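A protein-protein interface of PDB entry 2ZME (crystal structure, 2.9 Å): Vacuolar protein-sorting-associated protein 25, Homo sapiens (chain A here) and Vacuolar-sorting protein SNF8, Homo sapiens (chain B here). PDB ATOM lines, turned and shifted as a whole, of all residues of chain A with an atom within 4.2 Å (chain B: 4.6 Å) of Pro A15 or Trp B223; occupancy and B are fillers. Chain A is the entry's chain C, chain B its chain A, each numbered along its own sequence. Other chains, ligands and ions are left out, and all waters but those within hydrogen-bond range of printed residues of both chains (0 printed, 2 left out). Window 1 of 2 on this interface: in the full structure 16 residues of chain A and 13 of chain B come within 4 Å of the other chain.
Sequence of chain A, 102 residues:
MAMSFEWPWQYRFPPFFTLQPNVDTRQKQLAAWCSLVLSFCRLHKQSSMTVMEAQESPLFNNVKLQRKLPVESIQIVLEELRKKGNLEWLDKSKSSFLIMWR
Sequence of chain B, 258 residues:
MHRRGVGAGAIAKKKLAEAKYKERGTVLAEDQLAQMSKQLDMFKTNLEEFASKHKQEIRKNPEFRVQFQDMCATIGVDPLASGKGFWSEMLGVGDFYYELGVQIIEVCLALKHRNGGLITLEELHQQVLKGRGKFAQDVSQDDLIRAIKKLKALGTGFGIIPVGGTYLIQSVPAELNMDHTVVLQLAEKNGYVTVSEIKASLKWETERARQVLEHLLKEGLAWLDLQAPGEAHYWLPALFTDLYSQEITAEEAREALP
Printed residues of chain A that touch a printed residue of chain B: Phe A13, Pro A14, Pro A15, Thr A18, Gln A20 and Thr A25.
Hydrophobic or aromatic side chains of chain A within 4 Å of the printed part of chain B: Phe A13, Pro A14 and Pro A15.
Hydrophobic or aromatic side chains of chain B within 4 Å of the printed part of chain A: Trp B223, Leu B224 and Trp B235.
Of the printed residues of chain B, Phe A13 touches Trp B223 and Trp B235.
Of the printed residues of chain B, Pro A14 touches Asp B225 and Trp B235.
Pro A15 touches four residues of chain B.
Printed residues of chain B within 4 Å of Thr A18: Leu B224 (3.7 Å).
Leu B217 touches none of the printed residues of chain A.
Of the printed residues of chain A, Leu B224 touches Pro A15, Thr A18 and Gln A20.
Of the printed residues of chain A, Asp B225 touches Pro A14 (3.99 Å) and Pro A15 (3.96 Å).
His B233 touches none of the printed residues of chain A.
NE2 of Gln A20 is in hydrogen-bond range of O of Leu B224, at 2.7 Å.
Among the printed residues, merely in contact across the chains: Pro A15 with Leu B224 (2.9 Å), Gln A20 with Trp B223 (3.3 Å), Pro A15 with Trp B235 (3.3 Å), Thr A25 with Trp B223 (3.4 Å), Pro A15 with Trp B223 (3.5 Å), Pro A14 with Trp B235 (3.7 Å), Thr A18 with Leu B224 (3.7 Å), Phe A13 with Trp B223 (3.8 Å), Phe A13 with Trp B235 (3.8 Å), Pro A15 with Asp B225 (3.96 Å) and Pro A14 with Asp B225 (3.99 Å).
N of Trp B223 sits at hydrogen-bond distance from O of Trp B235.
The indole nitrogen (NE1) of Trp B235 sits at hydrogen-bond distance from the side-chain carboxylate (OD1) of Asp B225, at 2.9 Å.
The side-chain amide nitrogen (NE2) of Gln A20 lies within hydrogen-bond range of the backbone carbonyl oxygen (O) of Pro A15, 3.0 Å away.
The backbone carbonyl oxygen (O) of Thr A18 is in hydrogen-bond range of the side-chain amide nitrogen (NE2) of Gln A20, at 2.9 Å.
O of Thr A18 lies within hydrogen-bond range of NE2 of Gln A29.
OE1 of Gln A29 sits at hydrogen-bond distance from N of Gln A20, 3.0 Å away.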
ATOM      1  N   PHE A  13      16.550   4.488  21.164  1.00  0.00           N
ATOM      2  CA  PHE A  13      15.394   5.188  21.823  1.00  0.00           C
ATOM      3  C   PHE A  13      14.146   5.333  20.904  1.00  0.00           C
ATOM      4  O   PHE A  13      14.206   6.063  19.901  1.00  0.00           O
ATOM      5  CB  PHE A  13      15.876   6.554  22.329  1.00  0.00           C
ATOM      6  CG  PHE A  13      14.868   7.314  23.117  1.00  0.00           C
ATOM      7  CD1 PHE A  13      14.235   6.743  24.210  1.00  0.00           C
ATOM      8  CD2 PHE A  13      14.585   8.622  22.804  1.00  0.00           C
ATOM      9  CE1 PHE A  13      13.330   7.456  24.981  1.00  0.00           C
ATOM     10  CE2 PHE A  13      13.666   9.352  23.548  1.00  0.00           C
ATOM     11  CZ  PHE A  13      13.035   8.773  24.647  1.00  0.00           C
ATOM     12  N   PRO A  14      13.027   4.628  21.210  1.00  0.00           N
ATOM     13  CA  PRO A  14      11.923   4.566  20.243  1.00  0.00           C
ATOM     14  C   PRO A  14      11.524   5.888  19.545  1.00  0.00           C
ATOM     15  O   PRO A  14      11.453   5.913  18.312  1.00  0.00           O
ATOM     16  CB  PRO A  14      10.775   3.950  21.048  1.00  0.00           C
ATOM     17  CG  PRO A  14      11.443   3.036  21.940  1.00  0.00           C
ATOM     18  CD  PRO A  14      12.718   3.800  22.386  1.00  0.00           C
ATOM     19  N   PRO A  15      11.299   6.984  20.289  1.00  0.00           N
ATOM     20  CA  PRO A  15      10.774   8.133  19.536  1.00  0.00           C
ATOM     21  C   PRO A  15      11.787   8.830  18.629  1.00  0.00           C
ATOM     22  O   PRO A  15      11.431   9.732  17.879  1.00  0.00           O
ATOM     23  CB  PRO A  15      10.261   9.068  20.634  1.00  0.00           C
ATOM     24  CG  PRO A  15      10.264   8.229  21.956  1.00  0.00           C
ATOM     25  CD  PRO A  15      11.411   7.268  21.732  1.00  0.00           C
ATOM     26  N   PHE A  16      13.037   8.403  18.662  1.00  0.00           N
ATOM     27  CA  PHE A  16      14.041   8.956  17.765  1.00  0.00           C
ATOM     28  C   PHE A  16      13.591   8.676  16.325  1.00  0.00           C
ATOM     29  O   PHE A  16      14.121   9.260  15.347  1.00  0.00           O
ATOM     30  CB  PHE A  16      15.397   8.303  18.070  1.00  0.00           C
ATOM     31  CG  PHE A  16      16.557   8.801  17.231  1.00  0.00           C
ATOM     32  CD1 PHE A  16      16.979  10.139  17.292  1.00  0.00           C
ATOM     33  CD2 PHE A  16      17.266   7.910  16.404  1.00  0.00           C
ATOM     34  CE1 PHE A  16      18.069  10.593  16.523  1.00  0.00           C
ATOM     35  CE2 PHE A  16      18.378   8.335  15.608  1.00  0.00           C
ATOM     36  CZ  PHE A  16      18.779   9.679  15.664  1.00  0.00           C
ATOM     37  N   PHE A  17      12.622   7.757  16.186  1.00  0.00           N
ATOM     38  CA  PHE A  17      12.145   7.296  14.858  1.00  0.00           C
ATOM     39  C   PHE A  17      10.867   8.047  14.413  1.00  0.00           C
ATOM     40  O   PHE A  17      10.159   7.607  13.509  1.00  0.00           O
ATOM     41  CB  PHE A  17      12.005   5.763  14.832  1.00  0.00           C
ATOM     42  CG  PHE A  17      13.326   5.040  14.928  1.00  0.00           C
ATOM     43  CD1 PHE A  17      13.881   4.733  16.170  1.00  0.00           C
ATOM     44  CD2 PHE A  17      14.045   4.697  13.763  1.00  0.00           C
ATOM     45  CE1 PHE A  17      15.134   4.097  16.279  1.00  0.00           C
ATOM     46  CE2 PHE A  17      15.315   4.042  13.839  1.00  0.00           C
ATOM     47  CZ  PHE A  17      15.854   3.736  15.109  1.00  0.00           C
ATOM     48  N   THR A  18      10.629   9.200  15.032  1.00  0.00           N
ATOM     49  CA  THR A  18       9.477  10.023  14.793  1.00  0.00           C
ATOM     50  C   THR A  18       9.912  11.463  14.810  1.00  0.00           C
ATOM     51  O   THR A  18      10.451  11.952  15.810  1.00  0.00           O
ATOM     52  CB  THR A  18       8.487   9.876  15.919  1.00  0.00           C
ATOM     53  OG1 THR A  18       8.030   8.532  15.953  1.00  0.00           O
ATOM     54  CG2 THR A  18       7.311  10.761  15.732  1.00  0.00           C
ATOM     55  N   GLN A  20       9.930  15.077  15.508  1.00  0.00           N
ATOM     56  CA  GLN A  20       9.355  15.560  16.754  1.00  0.00           C
ATOM     57  C   GLN A  20       8.565  16.881  16.616  1.00  0.00           C
ATOM     58  O   GLN A  20       8.968  17.816  15.902  1.00  0.00           O
ATOM     59  CB  GLN A  20      10.433  15.618  17.847  1.00  0.00           C
ATOM     60  CG  GLN A  20      10.966  14.250  18.294  1.00  0.00           C
ATOM     61  CD  GLN A  20       9.914  13.423  19.033  1.00  0.00           C
ATOM     62  OE1 GLN A  20       9.254  13.929  19.949  1.00  0.00           O
ATOM     63  NE2 GLN A  20       9.741  12.145  18.633  1.00  0.00           N
ATOM     64  N   THR A  25      13.675  20.117  20.170  1.00  0.00           N
ATOM     65  CA  THR A  25      13.958  18.690  20.067  1.00  0.00           C
ATOM     66  C   THR A  25      14.128  18.170  18.618  1.00  0.00           C
ATOM     67  O   THR A  25      14.972  17.297  18.354  1.00  0.00           O
ATOM     68  CB  THR A  25      12.863  17.918  20.751  1.00  0.00           C
ATOM     69  OG1 THR A  25      12.467  18.646  21.919  1.00  0.00           O
ATOM     70  CG2 THR A  25      13.345  16.570  21.149  1.00  0.00           C
ATOM     71  N   GLN A  29      17.178  16.100  17.450  1.00  0.00           N
ATOM     72  CA  GLN A  29      16.969  14.861  16.708  1.00  0.00           C
ATOM     73  C   GLN A  29      17.679  14.886  15.328  1.00  0.00           C
ATOM     74  O   GLN A  29      18.471  13.978  15.009  1.00  0.00           O
ATOM     75  CB  GLN A  29      15.447  14.607  16.585  1.00  0.00           C
ATOM     76  CG  GLN A  29      15.013  13.500  15.646  1.00  0.00           C
ATOM     77  CD  GLN A  29      13.524  13.186  15.694  1.00  0.00           C
ATOM     78  OE1 GLN A  29      12.695  14.090  15.801  1.00  0.00           O
ATOM     79  NE2 GLN A  29      13.168  11.885  15.601  1.00  0.00           N
ATOM     80  N   LEU B 217       6.315  17.995  26.312  1.00  0.00           N
ATOM     81  CA  LEU B 217       7.012  18.000  25.018  1.00  0.00           C
ATOM     82  C   LEU B 217       7.633  19.374  24.781  1.00  0.00           C
ATOM     83  O   LEU B 217       8.760  19.498  24.285  1.00  0.00           O
ATOM     84  CB  LEU B 217       6.044  17.694  23.885  1.00  0.00           C
ATOM     85  CG  LEU B 217       5.466  16.298  23.694  1.00  0.00           C
ATOM     86  CD1 LEU B 217       4.217  16.354  22.770  1.00  0.00           C
ATOM     87  CD2 LEU B 217       6.555  15.347  23.162  1.00  0.00           C
ATOM     88  N   GLY B 220      10.943  19.777  26.525  1.00  0.00           N
ATOM     89  CA  GLY B 220      11.993  18.845  26.281  1.00  0.00           C
ATOM     90  C   GLY B 220      11.958  17.613  27.148  1.00  0.00           C
ATOM     91  O   GLY B 220      12.881  16.802  27.054  1.00  0.00           O
ATOM     92  N   ALA B 222       9.727  15.078  27.249  1.00  0.00           N
ATOM     93  CA  ALA B 222       9.191  13.871  26.649  1.00  0.00           C
ATOM     94  C   ALA B 222       9.373  13.882  25.111  1.00  0.00           C
ATOM     95  O   ALA B 222       9.778  14.879  24.536  1.00  0.00           O
ATOM     96  CB  ALA B 222       7.780  13.729  27.043  1.00  0.00           C
ATOM     97  N   TRP B 223       9.150  12.769  24.446  1.00  0.00           N
ATOM     98  CA  TRP B 223       9.344  12.702  23.009  1.00  0.00           C
ATOM     99  C   TRP B 223       8.172  11.889  22.517  1.00  0.00           C
ATOM    100  O   TRP B 223       7.852  10.850  23.117  1.00  0.00           O
ATOM    101  CB  TRP B 223      10.613  11.919  22.671  1.00  0.00           C
ATOM    102  CG  TRP B 223      11.936  12.660  22.814  1.00  0.00           C
ATOM    103  CD1 TRP B 223      12.366  13.379  23.896  1.00  0.00           C
ATOM    104  CD2 TRP B 223      13.005  12.710  21.853  1.00  0.00           C
ATOM    105  NE1 TRP B 223      13.624  13.871  23.667  1.00  0.00           N
ATOM    106  CE2 TRP B 223      14.046  13.489  22.428  1.00  0.00           C
ATOM    107  CE3 TRP B 223      13.182  12.174  20.570  1.00  0.00           C
ATOM    108  CZ2 TRP B 223      15.261  13.768  21.763  1.00  0.00           C
ATOM    109  CZ3 TRP B 223      14.397  12.459  19.888  1.00  0.00           C
ATOM    110  CH2 TRP B 223      15.424  13.258  20.504  1.00  0.00           C
ATOM    111  N   LEU B 224       7.529  12.358  21.445  1.00  0.00           N
ATOM    112  CA  LEU B 224       6.368  11.683  20.858  1.00  0.00           C
ATOM    113  C   LEU B 224       6.836  10.423  20.158  1.00  0.00           C
ATOM    114  O   LEU B 224       7.888  10.424  19.528  1.00  0.00           O
ATOM    115  CB  LEU B 224       5.647  12.598  19.845  1.00  0.00           C
ATOM    116  CG  LEU B 224       4.478  11.983  19.047  1.00  0.00           C
ATOM    117  CD1 LEU B 224       3.337  11.669  19.987  1.00  0.00           C
ATOM    118  CD2 LEU B 224       4.011  12.915  17.958  1.00  0.00           C
ATOM    119  N   ASP B 225       6.049   9.364  20.282  1.00  0.00           N
ATOM    120  CA  ASP B 225       6.282   8.144  19.539  1.00  0.00           C
ATOM    121  C   ASP B 225       5.021   7.637  18.806  1.00  0.00           C
ATOM    122  O   ASP B 225       4.077   7.196  19.483  1.00  0.00           O
ATOM    123  CB  ASP B 225       6.777   7.066  20.492  1.00  0.00           C
ATOM    124  CG  ASP B 225       6.836   5.691  19.842  1.00  0.00           C
ATOM    125  OD1 ASP B 225       6.879   4.687  20.594  1.00  0.00           O
ATOM    126  OD2 ASP B 225       6.830   5.622  18.580  1.00  0.00           O
ATOM    127  N   HIS B 233       2.578   7.075  22.066  1.00  0.00           N
ATOM    128  CA  HIS B 233       3.254   6.941  23.332  1.00  0.00           C
ATOM    129  C   HIS B 233       4.153   8.090  23.530  1.00  0.00           C
ATOM    130  O   HIS B 233       4.684   8.635  22.580  1.00  0.00           O
ATOM    131  CB  HIS B 233       4.097   5.703  23.290  1.00  0.00           C
ATOM    132  CG  HIS B 233       3.303   4.470  23.508  1.00  0.00           C
ATOM    133  ND1 HIS B 233       2.036   4.310  22.985  1.00  0.00           N
ATOM    134  CD2 HIS B 233       3.571   3.353  24.225  1.00  0.00           C
ATOM    135  CE1 HIS B 233       1.567   3.135  23.363  1.00  0.00           C
ATOM    136  NE2 HIS B 233       2.477   2.537  24.116  1.00  0.00           N
ATOM    137  N   TYR B 234       4.339   8.456  24.782  1.00  0.00           N
ATOM    138  CA  TYR B 234       5.084   9.643  25.098  1.00  0.00           C
ATOM    139  C   TYR B 234       6.108   9.122  26.021  1.00  0.00           C
ATOM    140  O   TYR B 234       5.751   8.688  27.128  1.00  0.00           O
ATOM    141  CB  TYR B 234       4.211  10.655  25.826  1.00  0.00           C
ATOM    142  CG  TYR B 234       3.130  11.238  24.956  1.00  0.00           C
ATOM    143  CD1 TYR B 234       2.048  10.476  24.577  1.00  0.00           C
ATOM    144  CD2 TYR B 234       3.201  12.543  24.513  1.00  0.00           C
ATOM    145  CE1 TYR B 234       1.078  10.972  23.797  1.00  0.00           C
ATOM    146  CE2 TYR B 234       2.214  13.079  23.709  1.00  0.00           C
ATOM    147  CZ  TYR B 234       1.141  12.278  23.347  1.00  0.00           C
ATOM    148  OH  TYR B 234       0.105  12.756  22.540  1.00  0.00           O
ATOM    149  N   TRP B 235       7.364   9.131  25.570  1.00  0.00           N
ATOM    150  CA  TRP B 235       8.453   8.603  26.349  1.00  0.00           C
ATOM    151  C   TRP B 235       9.215   9.729  26.994  1.00  0.00           C
ATOM    152  O   TRP B 235       9.480  10.712  26.335  1.00  0.00           O
ATOM    153  CB  TRP B 235       9.406   7.873  25.431  1.00  0.00           C
ATOM    154  CG  TRP B 235       8.822   6.718  24.743  1.00  0.00           C
ATOM    155  CD1 TRP B 235       7.890   6.736  23.752  1.00  0.00           C
ATOM    156  CD2 TRP B 235       9.148   5.344  24.968  1.00  0.00           C
ATOM    157  NE1 TRP B 235       7.612   5.450  23.341  1.00  0.00           N
ATOM    158  CE2 TRP B 235       8.369   4.579  24.081  1.00  0.00           C
ATOM    159  CE3 TRP B 235      10.005   4.684  25.843  1.00  0.00           C
ATOM    160  CZ2 TRP B 235       8.425   3.184  24.059  1.00  0.00           C
ATOM    161  CZ3 TRP B 235      10.052   3.307  25.810  1.00  0.00           C
ATOM    162  CH2 TRP B 235       9.270   2.575  24.936  1.00  0.00           C
ATOM    163  N   PRO B 237      12.798  10.571  28.498  1.00  0.00           N
ATOM    164  CA  PRO B 237      14.102   9.897  28.547  1.00  0.00           C
ATOM    165  C   PRO B 237      14.674   9.774  29.972  1.00  0.00           C
ATOM    166  O   PRO B 237      15.554   8.955  30.190  1.00  0.00           O
ATOM    167  CB  PRO B 237      15.001  10.793  27.696  1.00  0.00           C
ATOM    168  CG  PRO B 237      14.120  11.819  27.058  1.00  0.00           C
ATOM    169  CD  PRO B 237      12.848  11.879  27.821  1.00  0.00           C
